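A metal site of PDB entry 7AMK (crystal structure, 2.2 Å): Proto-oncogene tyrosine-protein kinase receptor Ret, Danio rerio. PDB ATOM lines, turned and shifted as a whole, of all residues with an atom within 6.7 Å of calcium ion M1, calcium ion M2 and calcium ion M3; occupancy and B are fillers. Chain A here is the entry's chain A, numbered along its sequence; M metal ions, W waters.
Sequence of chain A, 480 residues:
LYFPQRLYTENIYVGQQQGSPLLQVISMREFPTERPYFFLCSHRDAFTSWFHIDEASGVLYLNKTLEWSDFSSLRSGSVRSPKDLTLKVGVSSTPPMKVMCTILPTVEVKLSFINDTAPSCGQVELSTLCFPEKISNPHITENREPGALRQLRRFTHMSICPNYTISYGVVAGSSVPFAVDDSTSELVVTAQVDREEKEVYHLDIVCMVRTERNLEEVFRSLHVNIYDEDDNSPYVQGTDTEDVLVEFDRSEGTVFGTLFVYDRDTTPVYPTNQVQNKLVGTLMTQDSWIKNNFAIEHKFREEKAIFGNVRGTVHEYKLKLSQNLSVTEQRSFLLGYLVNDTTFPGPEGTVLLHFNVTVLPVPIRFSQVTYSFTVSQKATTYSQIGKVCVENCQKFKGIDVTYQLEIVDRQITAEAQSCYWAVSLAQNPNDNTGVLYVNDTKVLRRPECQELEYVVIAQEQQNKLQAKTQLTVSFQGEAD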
ATOM      1  N   GLU A 142     -13.814  19.671 -32.012  1.00  0.00           N
ATOM      2  CA  GLU A 142     -14.663  19.811 -33.194  1.00  0.00           C
ATOM      3  C   GLU A 142     -14.472  21.202 -33.820  1.00  0.00           C
ATOM      4  O   GLU A 142     -13.921  22.122 -33.206  1.00  0.00           O
ATOM      5  CB  GLU A 142     -16.131  19.564 -32.783  1.00  0.00           C
ATOM      6  CG  GLU A 142     -16.666  20.576 -31.803  1.00  0.00           C
ATOM      7  CD  GLU A 142     -18.179  20.566 -31.661  1.00  0.00           C
ATOM      8  OE1 GLU A 142     -18.883  20.002 -32.520  1.00  0.00           O
ATOM      9  OE2 GLU A 142     -18.643  21.123 -30.655  1.00  0.00           O
ATOM     10  N   ASN A 143     -14.893  21.324 -35.087  1.00  0.00           N
ATOM     11  CA  ASN A 143     -14.932  22.624 -35.791  1.00  0.00           C
ATOM     12  C   ASN A 143     -13.551  23.299 -35.888  1.00  0.00           C
ATOM     13  O   ASN A 143     -13.433  24.510 -35.737  1.00  0.00           O
ATOM     14  CB  ASN A 143     -15.912  23.606 -35.149  1.00  0.00           C
ATOM     15  CG  ASN A 143     -17.302  23.038 -35.001  1.00  0.00           C
ATOM     16  OD1 ASN A 143     -17.745  22.232 -35.814  1.00  0.00           O
ATOM     17  ND2 ASN A 143     -17.999  23.451 -33.959  1.00  0.00           N
ATOM     18  N   VAL A 193     -14.513  18.176 -37.866  1.00  0.00           N
ATOM     19  CA  VAL A 193     -15.432  17.144 -37.407  1.00  0.00           C
ATOM     20  C   VAL A 193     -16.489  17.791 -36.494  1.00  0.00           C
ATOM     21  O   VAL A 193     -16.405  18.968 -36.147  1.00  0.00           O
ATOM     22  CB  VAL A 193     -14.679  15.999 -36.703  1.00  0.00           C
ATOM     23  CG1 VAL A 193     -13.651  15.459 -37.674  1.00  0.00           C
ATOM     24  CG2 VAL A 193     -13.970  16.495 -35.411  1.00  0.00           C
ATOM     25  N   ASP A 194     -17.502  16.999 -36.152  1.00  0.00           N
ATOM     26  CA  ASP A 194     -18.674  17.477 -35.408  1.00  0.00           C
ATOM     27  C   ASP A 194     -18.852  16.556 -34.216  1.00  0.00           C
ATOM     28  O   ASP A 194     -19.213  15.382 -34.362  1.00  0.00           O
ATOM     29  CB  ASP A 194     -19.914  17.509 -36.318  1.00  0.00           C
ATOM     30  CG  ASP A 194     -21.205  17.992 -35.595  1.00  0.00           C
ATOM     31  OD1 ASP A 194     -21.129  18.480 -34.452  1.00  0.00           O
ATOM     32  OD2 ASP A 194     -22.307  17.850 -36.167  1.00  0.00           O
ATOM     33  N   ARG A 195     -18.566  17.084 -33.020  1.00  0.00           N
ATOM     34  CA  ARG A 195     -18.696  16.280 -31.817  1.00  0.00           C
ATOM     35  C   ARG A 195     -20.120  15.717 -31.726  1.00  0.00           C
ATOM     36  O   ARG A 195     -20.313  14.574 -31.279  1.00  0.00           O
ATOM     37  CB  ARG A 195     -18.344  17.116 -30.584  1.00  0.00           C
ATOM     38  CG  ARG A 195     -18.104  16.317 -29.297  1.00  0.00           C
ATOM     39  CD  ARG A 195     -19.369  15.698 -28.693  1.00  0.00           C
ATOM     40  NE  ARG A 195     -20.378  16.697 -28.385  1.00  0.00           N
ATOM     41  CZ  ARG A 195     -21.507  16.487 -27.716  1.00  0.00           C
ATOM     42  NH1 ARG A 195     -21.821  15.302 -27.214  1.00  0.00           N
ATOM     43  NH2 ARG A 195     -22.355  17.496 -27.548  1.00  0.00           N
ATOM     44  N   GLU A 196     -21.116  16.478 -32.176  1.00  0.00           N
ATOM     45  CA  GLU A 196     -22.508  16.038 -32.100  1.00  0.00           C
ATOM     46  C   GLU A 196     -22.816  14.908 -33.063  1.00  0.00           C
ATOM     47  O   GLU A 196     -23.823  14.206 -32.892  1.00  0.00           O
ATOM     48  CB  GLU A 196     -23.468  17.209 -32.360  1.00  0.00           C
ATOM     49  CG  GLU A 196     -23.778  18.074 -31.114  1.00  0.00           C
ATOM     50  CD  GLU A 196     -22.652  19.055 -30.737  1.00  0.00           C
ATOM     51  OE1 GLU A 196     -21.981  19.587 -31.647  1.00  0.00           O
ATOM     52  OE2 GLU A 196     -22.452  19.302 -29.521  1.00  0.00           O
ATOM     53  N   GLU A 197     -22.014  14.706 -34.090  1.00  0.00           N
ATOM     54  CA  GLU A 197     -22.213  13.536 -34.928  1.00  0.00           C
ATOM     55  C   GLU A 197     -21.472  12.338 -34.373  1.00  0.00           C
ATOM     56  O   GLU A 197     -22.029  11.236 -34.331  1.00  0.00           O
ATOM     57  CB  GLU A 197     -21.766  13.806 -36.368  1.00  0.00           C
ATOM     58  N   TYR A 227     -13.319  16.568 -28.752  1.00  0.00           N
ATOM     59  CA  TYR A 227     -13.746  17.507 -27.722  1.00  0.00           C
ATOM     60  C   TYR A 227     -14.800  18.464 -28.247  1.00  0.00           C
ATOM     61  O   TYR A 227     -14.830  18.822 -29.419  1.00  0.00           O
ATOM     62  CB  TYR A 227     -12.554  18.308 -27.184  1.00  0.00           C
ATOM     63  CG  TYR A 227     -11.638  17.499 -26.306  1.00  0.00           C
ATOM     64  CD1 TYR A 227     -11.880  16.154 -26.034  1.00  0.00           C
ATOM     65  CD2 TYR A 227     -10.529  18.089 -25.729  1.00  0.00           C
ATOM     66  CE1 TYR A 227     -11.026  15.414 -25.207  1.00  0.00           C
ATOM     67  CE2 TYR A 227      -9.678  17.377 -24.908  1.00  0.00           C
ATOM     68  CZ  TYR A 227      -9.920  16.041 -24.656  1.00  0.00           C
ATOM     69  OH  TYR A 227      -9.031  15.372 -23.856  1.00  0.00           O
ATOM     70  N   ASP A 228     -15.661  18.895 -27.339  1.00  0.00           N
ATOM     71  CA  ASP A 228     -16.853  19.658 -27.647  1.00  0.00           C
ATOM     72  C   ASP A 228     -16.551  21.134 -27.531  1.00  0.00           C
ATOM     73  O   ASP A 228     -15.746  21.574 -26.706  1.00  0.00           O
ATOM     74  CB  ASP A 228     -17.974  19.281 -26.682  1.00  0.00           C
ATOM     75  CG  ASP A 228     -19.290  19.881 -27.043  1.00  0.00           C
ATOM     76  OD1 ASP A 228     -19.780  19.572 -28.133  1.00  0.00           O
ATOM     77  OD2 ASP A 228     -19.852  20.636 -26.234  1.00  0.00           O
ATOM     78  N   GLU A 229     -17.221  21.922 -28.351  1.00  0.00           N
ATOM     79  CA  GLU A 229     -17.261  23.354 -28.134  1.00  0.00           C
ATOM     80  C   GLU A 229     -18.713  23.806 -28.129  1.00  0.00           C
ATOM     81  O   GLU A 229     -19.616  23.040 -28.489  1.00  0.00           O
ATOM     82  CB  GLU A 229     -16.438  24.108 -29.181  1.00  0.00           C
ATOM     83  CG  GLU A 229     -17.083  24.231 -30.506  1.00  0.00           C
ATOM     84  CD  GLU A 229     -16.275  25.121 -31.439  1.00  0.00           C
ATOM     85  OE1 GLU A 229     -15.160  25.528 -31.043  1.00  0.00           O
ATOM     86  OE2 GLU A 229     -16.733  25.426 -32.574  1.00  0.00           O
ATOM     87  N   ASP A 230     -18.943  25.035 -27.686  1.00  0.00           N
ATOM     88  CA  ASP A 230     -20.295  25.564 -27.526  1.00  0.00           C
ATOM     89  C   ASP A 230     -20.743  26.068 -28.893  1.00  0.00           C
ATOM     90  O   ASP A 230     -20.457  27.198 -29.283  1.00  0.00           O
ATOM     91  CB  ASP A 230     -20.316  26.649 -26.444  1.00  0.00           C
ATOM     92  CG  ASP A 230     -21.720  27.251 -26.205  1.00  0.00           C
ATOM     93  OD1 ASP A 230     -22.728  26.801 -26.785  1.00  0.00           O
ATOM     94  OD2 ASP A 230     -21.789  28.215 -25.419  1.00  0.00           O
ATOM     95  N   ASP A 231     -21.416  25.202 -29.654  1.00  0.00           N
ATOM     96  CA  ASP A 231     -21.829  25.560 -31.007  1.00  0.00           C
ATOM     97  C   ASP A 231     -23.302  25.243 -31.229  1.00  0.00           C
ATOM     98  O   ASP A 231     -23.729  25.093 -32.383  1.00  0.00           O
ATOM     99  CB  ASP A 231     -20.930  24.871 -32.058  1.00  0.00           C
ATOM    100  CG  ASP A 231     -21.086  23.326 -32.065  1.00  0.00           C
ATOM    101  OD1 ASP A 231     -21.815  22.756 -31.228  1.00  0.00           O
ATOM    102  OD2 ASP A 231     -20.463  22.685 -32.938  1.00  0.00           O
ATOM    103  N   ASN A 232     -24.085  25.128 -30.160  1.00  0.00           N
ATOM    104  CA  ASN A 232     -25.513  24.912 -30.261  1.00  0.00           C
ATOM    105  C   ASN A 232     -26.219  25.835 -29.282  1.00  0.00           C
ATOM    106  O   ASN A 232     -25.828  25.925 -28.122  1.00  0.00           O
ATOM    107  CB  ASN A 232     -25.879  23.451 -29.969  1.00  0.00           C
ATOM    108  CG  ASN A 232     -25.392  22.504 -31.052  1.00  0.00           C
ATOM    109  OD1 ASN A 232     -26.090  22.248 -32.027  1.00  0.00           O
ATOM    110  ND2 ASN A 232     -24.178  21.985 -30.884  1.00  0.00           N
ATOM    111  N   SER A 233     -27.253  26.547 -29.770  1.00  0.00           N
ATOM    112  CA  SER A 233     -27.967  27.419 -28.875  1.00  0.00           C
ATOM    113  C   SER A 233     -29.036  26.658 -28.093  1.00  0.00           C
ATOM    114  O   SER A 233     -29.551  25.645 -28.563  1.00  0.00           O
ATOM    115  CB  SER A 233     -28.630  28.550 -29.641  1.00  0.00           C
ATOM    116  OG  SER A 233     -29.405  28.034 -30.695  1.00  0.00           O
ATOM    117  N   PRO A 234     -29.353  27.144 -26.899  1.00  0.00           N
ATOM    118  CA  PRO A 234     -30.424  26.522 -26.115  1.00  0.00           C
ATOM    119  C   PRO A 234     -31.774  26.748 -26.763  1.00  0.00           C
ATOM    120  O   PRO A 234     -31.980  27.672 -27.530  1.00  0.00           O
ATOM    121  CB  PRO A 234     -30.316  27.239 -24.768  1.00  0.00           C
ATOM    122  CG  PRO A 234     -29.711  28.562 -25.117  1.00  0.00           C
ATOM    123  CD  PRO A 234     -28.719  28.257 -26.189  1.00  0.00           C
ATOM    124  N   ASP A 263     -29.874  21.914 -24.547  1.00  0.00           N
ATOM    125  CA  ASP A 263     -28.698  22.369 -25.278  1.00  0.00           C
ATOM    126  C   ASP A 263     -27.914  21.131 -25.698  1.00  0.00           C
ATOM    127  O   ASP A 263     -27.549  20.313 -24.856  1.00  0.00           O
ATOM    128  CB  ASP A 263     -27.843  23.302 -24.402  1.00  0.00           C
ATOM    129  CG  ASP A 263     -26.800  24.075 -25.189  1.00  0.00           C
ATOM    130  OD1 ASP A 263     -26.090  23.478 -26.002  1.00  0.00           O
ATOM    131  OD2 ASP A 263     -26.681  25.293 -24.981  1.00  0.00           O
ATOM    132  N   ARG A 264     -27.680  20.983 -27.004  1.00  0.00           N
ATOM    133  CA  ARG A 264     -27.008  19.783 -27.495  1.00  0.00           C
ATOM    134  C   ARG A 264     -25.544  19.708 -27.077  1.00  0.00           C
ATOM    135  O   ARG A 264     -24.960  18.612 -27.112  1.00  0.00           O
ATOM    136  CB  ARG A 264     -27.133  19.696 -29.006  1.00  0.00           C
ATOM    137  CG  ARG A 264     -28.582  19.550 -29.435  1.00  0.00           C
ATOM    138  CD  ARG A 264     -28.732  19.254 -30.927  1.00  0.00           C
ATOM    139  NE  ARG A 264     -30.147  19.098 -31.262  1.00  0.00           N
ATOM    140  CZ  ARG A 264     -30.845  17.973 -31.140  1.00  0.00           C
ATOM    141  NH1 ARG A 264     -30.279  16.856 -30.724  1.00  0.00           N
ATOM    142  NH2 ARG A 264     -32.139  17.982 -31.446  1.00  0.00           N
ATOM    143  N   ASP A 265     -24.945  20.824 -26.692  1.00  0.00           N
ATOM    144  CA  ASP A 265     -23.575  20.831 -26.206  1.00  0.00           C
ATOM    145  C   ASP A 265     -23.484  20.223 -24.797  1.00  0.00           C
ATOM    146  O   ASP A 265     -24.434  20.256 -24.014  1.00  0.00           O
ATOM    147  CB  ASP A 265     -23.021  22.254 -26.190  1.00  0.00           C
ATOM    148  CG  ASP A 265     -23.027  22.895 -27.559  1.00  0.00           C
ATOM    149  OD1 ASP A 265     -22.682  22.202 -28.535  1.00  0.00           O
ATOM    150  OD2 ASP A 265     -23.388  24.084 -27.669  1.00  0.00           O
ATOM    151  N   THR A 266     -22.315  19.677 -24.489  1.00  0.00           N
ATOM    152  CA  THR A 266     -22.016  19.132 -23.170  1.00  0.00           C
ATOM    153  C   THR A 266     -21.565  20.229 -22.219  1.00  0.00           C
ATOM    154  O   THR A 266     -21.146  21.317 -22.619  1.00  0.00           O
ATOM    155  CB  THR A 266     -20.907  18.060 -23.250  1.00  0.00           C
ATOM    156  OG1 THR A 266     -19.652  18.695 -23.490  1.00  0.00           O
ATOM    157  CG2 THR A 266     -21.199  17.081 -24.374  1.00  0.00           C
ATOM    158  N   GLN A 276     -17.516  27.641 -20.454  1.00  0.00           N
ATOM    159  CA  GLN A 276     -18.000  27.054 -21.697  1.00  0.00           C
ATOM    160  C   GLN A 276     -19.420  26.542 -21.547  1.00  0.00           C
ATOM    161  O   GLN A 276     -19.705  25.686 -20.705  1.00  0.00           O
ATOM    162  CB  GLN A 276     -17.085  25.910 -22.143  1.00  0.00           C
ATOM    163  CG  GLN A 276     -17.765  24.916 -23.093  1.00  0.00           C
ATOM    164  CD  GLN A 276     -16.797  23.978 -23.817  1.00  0.00           C
ATOM    165  OE1 GLN A 276     -15.567  24.125 -23.744  1.00  0.00           O
ATOM    166  NE2 GLN A 276     -17.350  23.007 -24.544  1.00  0.00           N
ATOM    167  N   ASN A 277     -20.316  27.056 -22.382  1.00  0.00           N
ATOM    168  CA  ASN A 277     -21.681  26.547 -22.449  1.00  0.00           C
ATOM    169  C   ASN A 277     -22.485  26.868 -21.207  1.00  0.00           C
ATOM    170  O   ASN A 277     -23.543  26.294 -20.999  1.00  0.00           O
ATOM    171  CB  ASN A 277     -21.728  25.037 -22.682  1.00  0.00           C
ATOM    172  CG  ASN A 277     -22.929  24.635 -23.467  1.00  0.00           C
ATOM    173  OD1 ASN A 277     -23.295  25.318 -24.413  1.00  0.00           O
ATOM    174  ND2 ASN A 277     -23.591  23.562 -23.063  1.00  0.00           N
ATOM    175  N   LEU A 279     -25.112  28.749 -19.182  1.00  0.00           N
ATOM    176  CA  LEU A 279     -26.266  29.614 -19.364  1.00  0.00           C
ATOM    177  C   LEU A 279     -26.464  30.470 -18.108  1.00  0.00           C
ATOM    178  O   LEU A 279     -26.597  29.939 -17.013  1.00  0.00           O
ATOM    179  CB  LEU A 279     -27.547  28.808 -19.627  1.00  0.00           C
ATOM    180  CG  LEU A 279     -27.546  27.779 -20.766  1.00  0.00           C
ATOM    181  CD1 LEU A 279     -28.938  27.116 -20.881  1.00  0.00           C
ATOM    182  CD2 LEU A 279     -27.144  28.483 -22.033  1.00  0.00           C
ATOM    183  N   ASP A 341     -26.968  31.792 -23.385  1.00  0.00           N
ATOM    184  CA  ASP A 341     -25.785  30.952 -23.618  1.00  0.00           C
ATOM    185  C   ASP A 341     -24.606  31.869 -23.931  1.00  0.00           C
ATOM    186  O   ASP A 341     -24.436  32.304 -25.072  1.00  0.00           O
ATOM    187  CB  ASP A 341     -26.036  29.975 -24.751  1.00  0.00           C
ATOM    188  CG  ASP A 341     -24.860  28.986 -24.961  1.00  0.00           C
ATOM    189  OD1 ASP A 341     -23.735  29.190 -24.414  1.00  0.00           O
ATOM    190  OD2 ASP A 341     -25.102  27.982 -25.675  1.00  0.00           O
ATOM    191  N   THR A 343     -21.223  31.843 -24.184  1.00  0.00           N
ATOM    192  CA  THR A 343     -20.167  31.538 -25.132  1.00  0.00           C
ATOM    193  C   THR A 343     -20.685  31.046 -26.478  1.00  0.00           C
ATOM    194  O   THR A 343     -19.895  30.547 -27.285  1.00  0.00           O
ATOM    195  CB  THR A 343     -19.197  30.487 -24.543  1.00  0.00           C
ATOM    196  OG1 THR A 343     -19.938  29.360 -24.090  1.00  0.00           O
ATOM    197  CG2 THR A 343     -18.445  31.055 -23.360  1.00  0.00           C
ATOM    198  N   PHE A 344     -21.989  31.126 -26.731  1.00  0.00           N
ATOM    199  CA  PHE A 344     -22.477  30.780 -28.062  1.00  0.00           C
ATOM    200  C   PHE A 344     -22.232  31.948 -29.018  1.00  0.00           C
ATOM    201  O   PHE A 344     -22.716  33.055 -28.765  1.00  0.00           O
ATOM    202  CB  PHE A 344     -23.947  30.406 -28.044  1.00  0.00           C
ATOM    203  CG  PHE A 344     -24.489  30.069 -29.405  1.00  0.00           C
ATOM    204  CD1 PHE A 344     -24.277  28.822 -29.970  1.00  0.00           C
ATOM    205  CD2 PHE A 344     -25.188  31.023 -30.136  1.00  0.00           C
ATOM    206  CE1 PHE A 344     -24.759  28.514 -31.239  1.00  0.00           C
ATOM    207  CE2 PHE A 344     -25.688  30.715 -31.394  1.00  0.00           C
ATOM    208  CZ  PHE A 344     -25.469  29.472 -31.948  1.00  0.00           C
HETATM  209 CA    CA M   1     -24.628  25.561 -26.237  1.00  0.00          CA
HETATM  210 CA    CA M   2     -20.773  21.245 -29.600  1.00  0.00          CA
HETATM  211 CA    CA M   3     -20.902  20.522 -33.441  1.00  0.00          CA
HETATM  212  O   HOH W   1     -19.754  21.067 -35.392  1.00  0.00           O
HETATM  213  O   HOH W   2     -23.027  21.105 -34.217  1.00  0.00           O
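Calcium ion M2 is bound by the side-chain carboxylate (OE2) of Glu 142, the side-chain carboxylate (OD1) of Asp 265, the backbone carbonyl oxygen (O) of Glu 229, the side-chain carboxylate (OD1) of Asp 228, the side-chain carboxylate (OD1) of Asp 231, the side-chain carboxylate (OE2) of Glu 196 and the side-chain carboxylate (OE1) of Glu 196.
O of Asn 232 binds calcium ion M1, at 2.3 Å. Calcium ion M1 is bound by OD1 of Asn 277, at 2.3 Å. The side-chain carboxylate (OD1) of Asp 230 is bound to calcium ion M1 (2.3 Å). OD2 of Asp 265 binds calcium ion M1 (2.4 Å). The side-chain carboxylate (OD2) of Asp 263 is bound to calcium ion M1, 2.4 Å away. OD2 of Asp 341 is bound to calcium ion M1 (2.5 Å). Calcium ion M1 is bound by OD1 of Asp 263. Calcium ion M1 has seven donor atoms within binding distance.
Calcium ion M3 is bound by OD2 of Asp 231, OE1 of Glu 142, OD1 of Asp 194, OE1 of Glu 196, water W1 and water W2. Calcium ion M3 has six donor atoms within binding distance.
The side-chain carboxylate (OE1) of Glu 196 sits close to the side-chain amide nitrogen (ND2) of Asn 232 (3.3 Å). The backbone NH of Glu 142 sits at hydrogen-bond distance from the backbone carbonyl oxygen of Tyr 227 (2.9 Å). NH2 of Arg 195 lies close to OE2 of Glu 196. The side-chain carboxylate (OD2) of Asp 230 sits at hydrogen-bond distance from the backbone NH (N) of Phe 344 (3.2 Å). OD2 of Asp 230 lies within hydrogen-bond range of OG1 of Thr 343 (2.6 Å). The side-chain carboxylate of Glu 229 is in hydrogen-bond range of the side-chain amide nitrogen of Asn 143. N of Thr 266 lies within hydrogen-bond range of OD2 of Asp 228 (3.2 Å). The backbone NH (N) of Phe 344 sits at hydrogen-bond distance from the side-chain carboxylate (OD1) of Asp 341.
Seven residues have an atom within 4 Å of calcium ion M2: Glu 142, Glu 196, Asp 228, Glu 229, Asp 231, Asn 232 and Asp 265.
Of the 25 residues printed, 4 come within 4 Å of calcium ion M3. Along chain A the residues within 4 Å of calcium ion M3 span positions 142 to 231.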
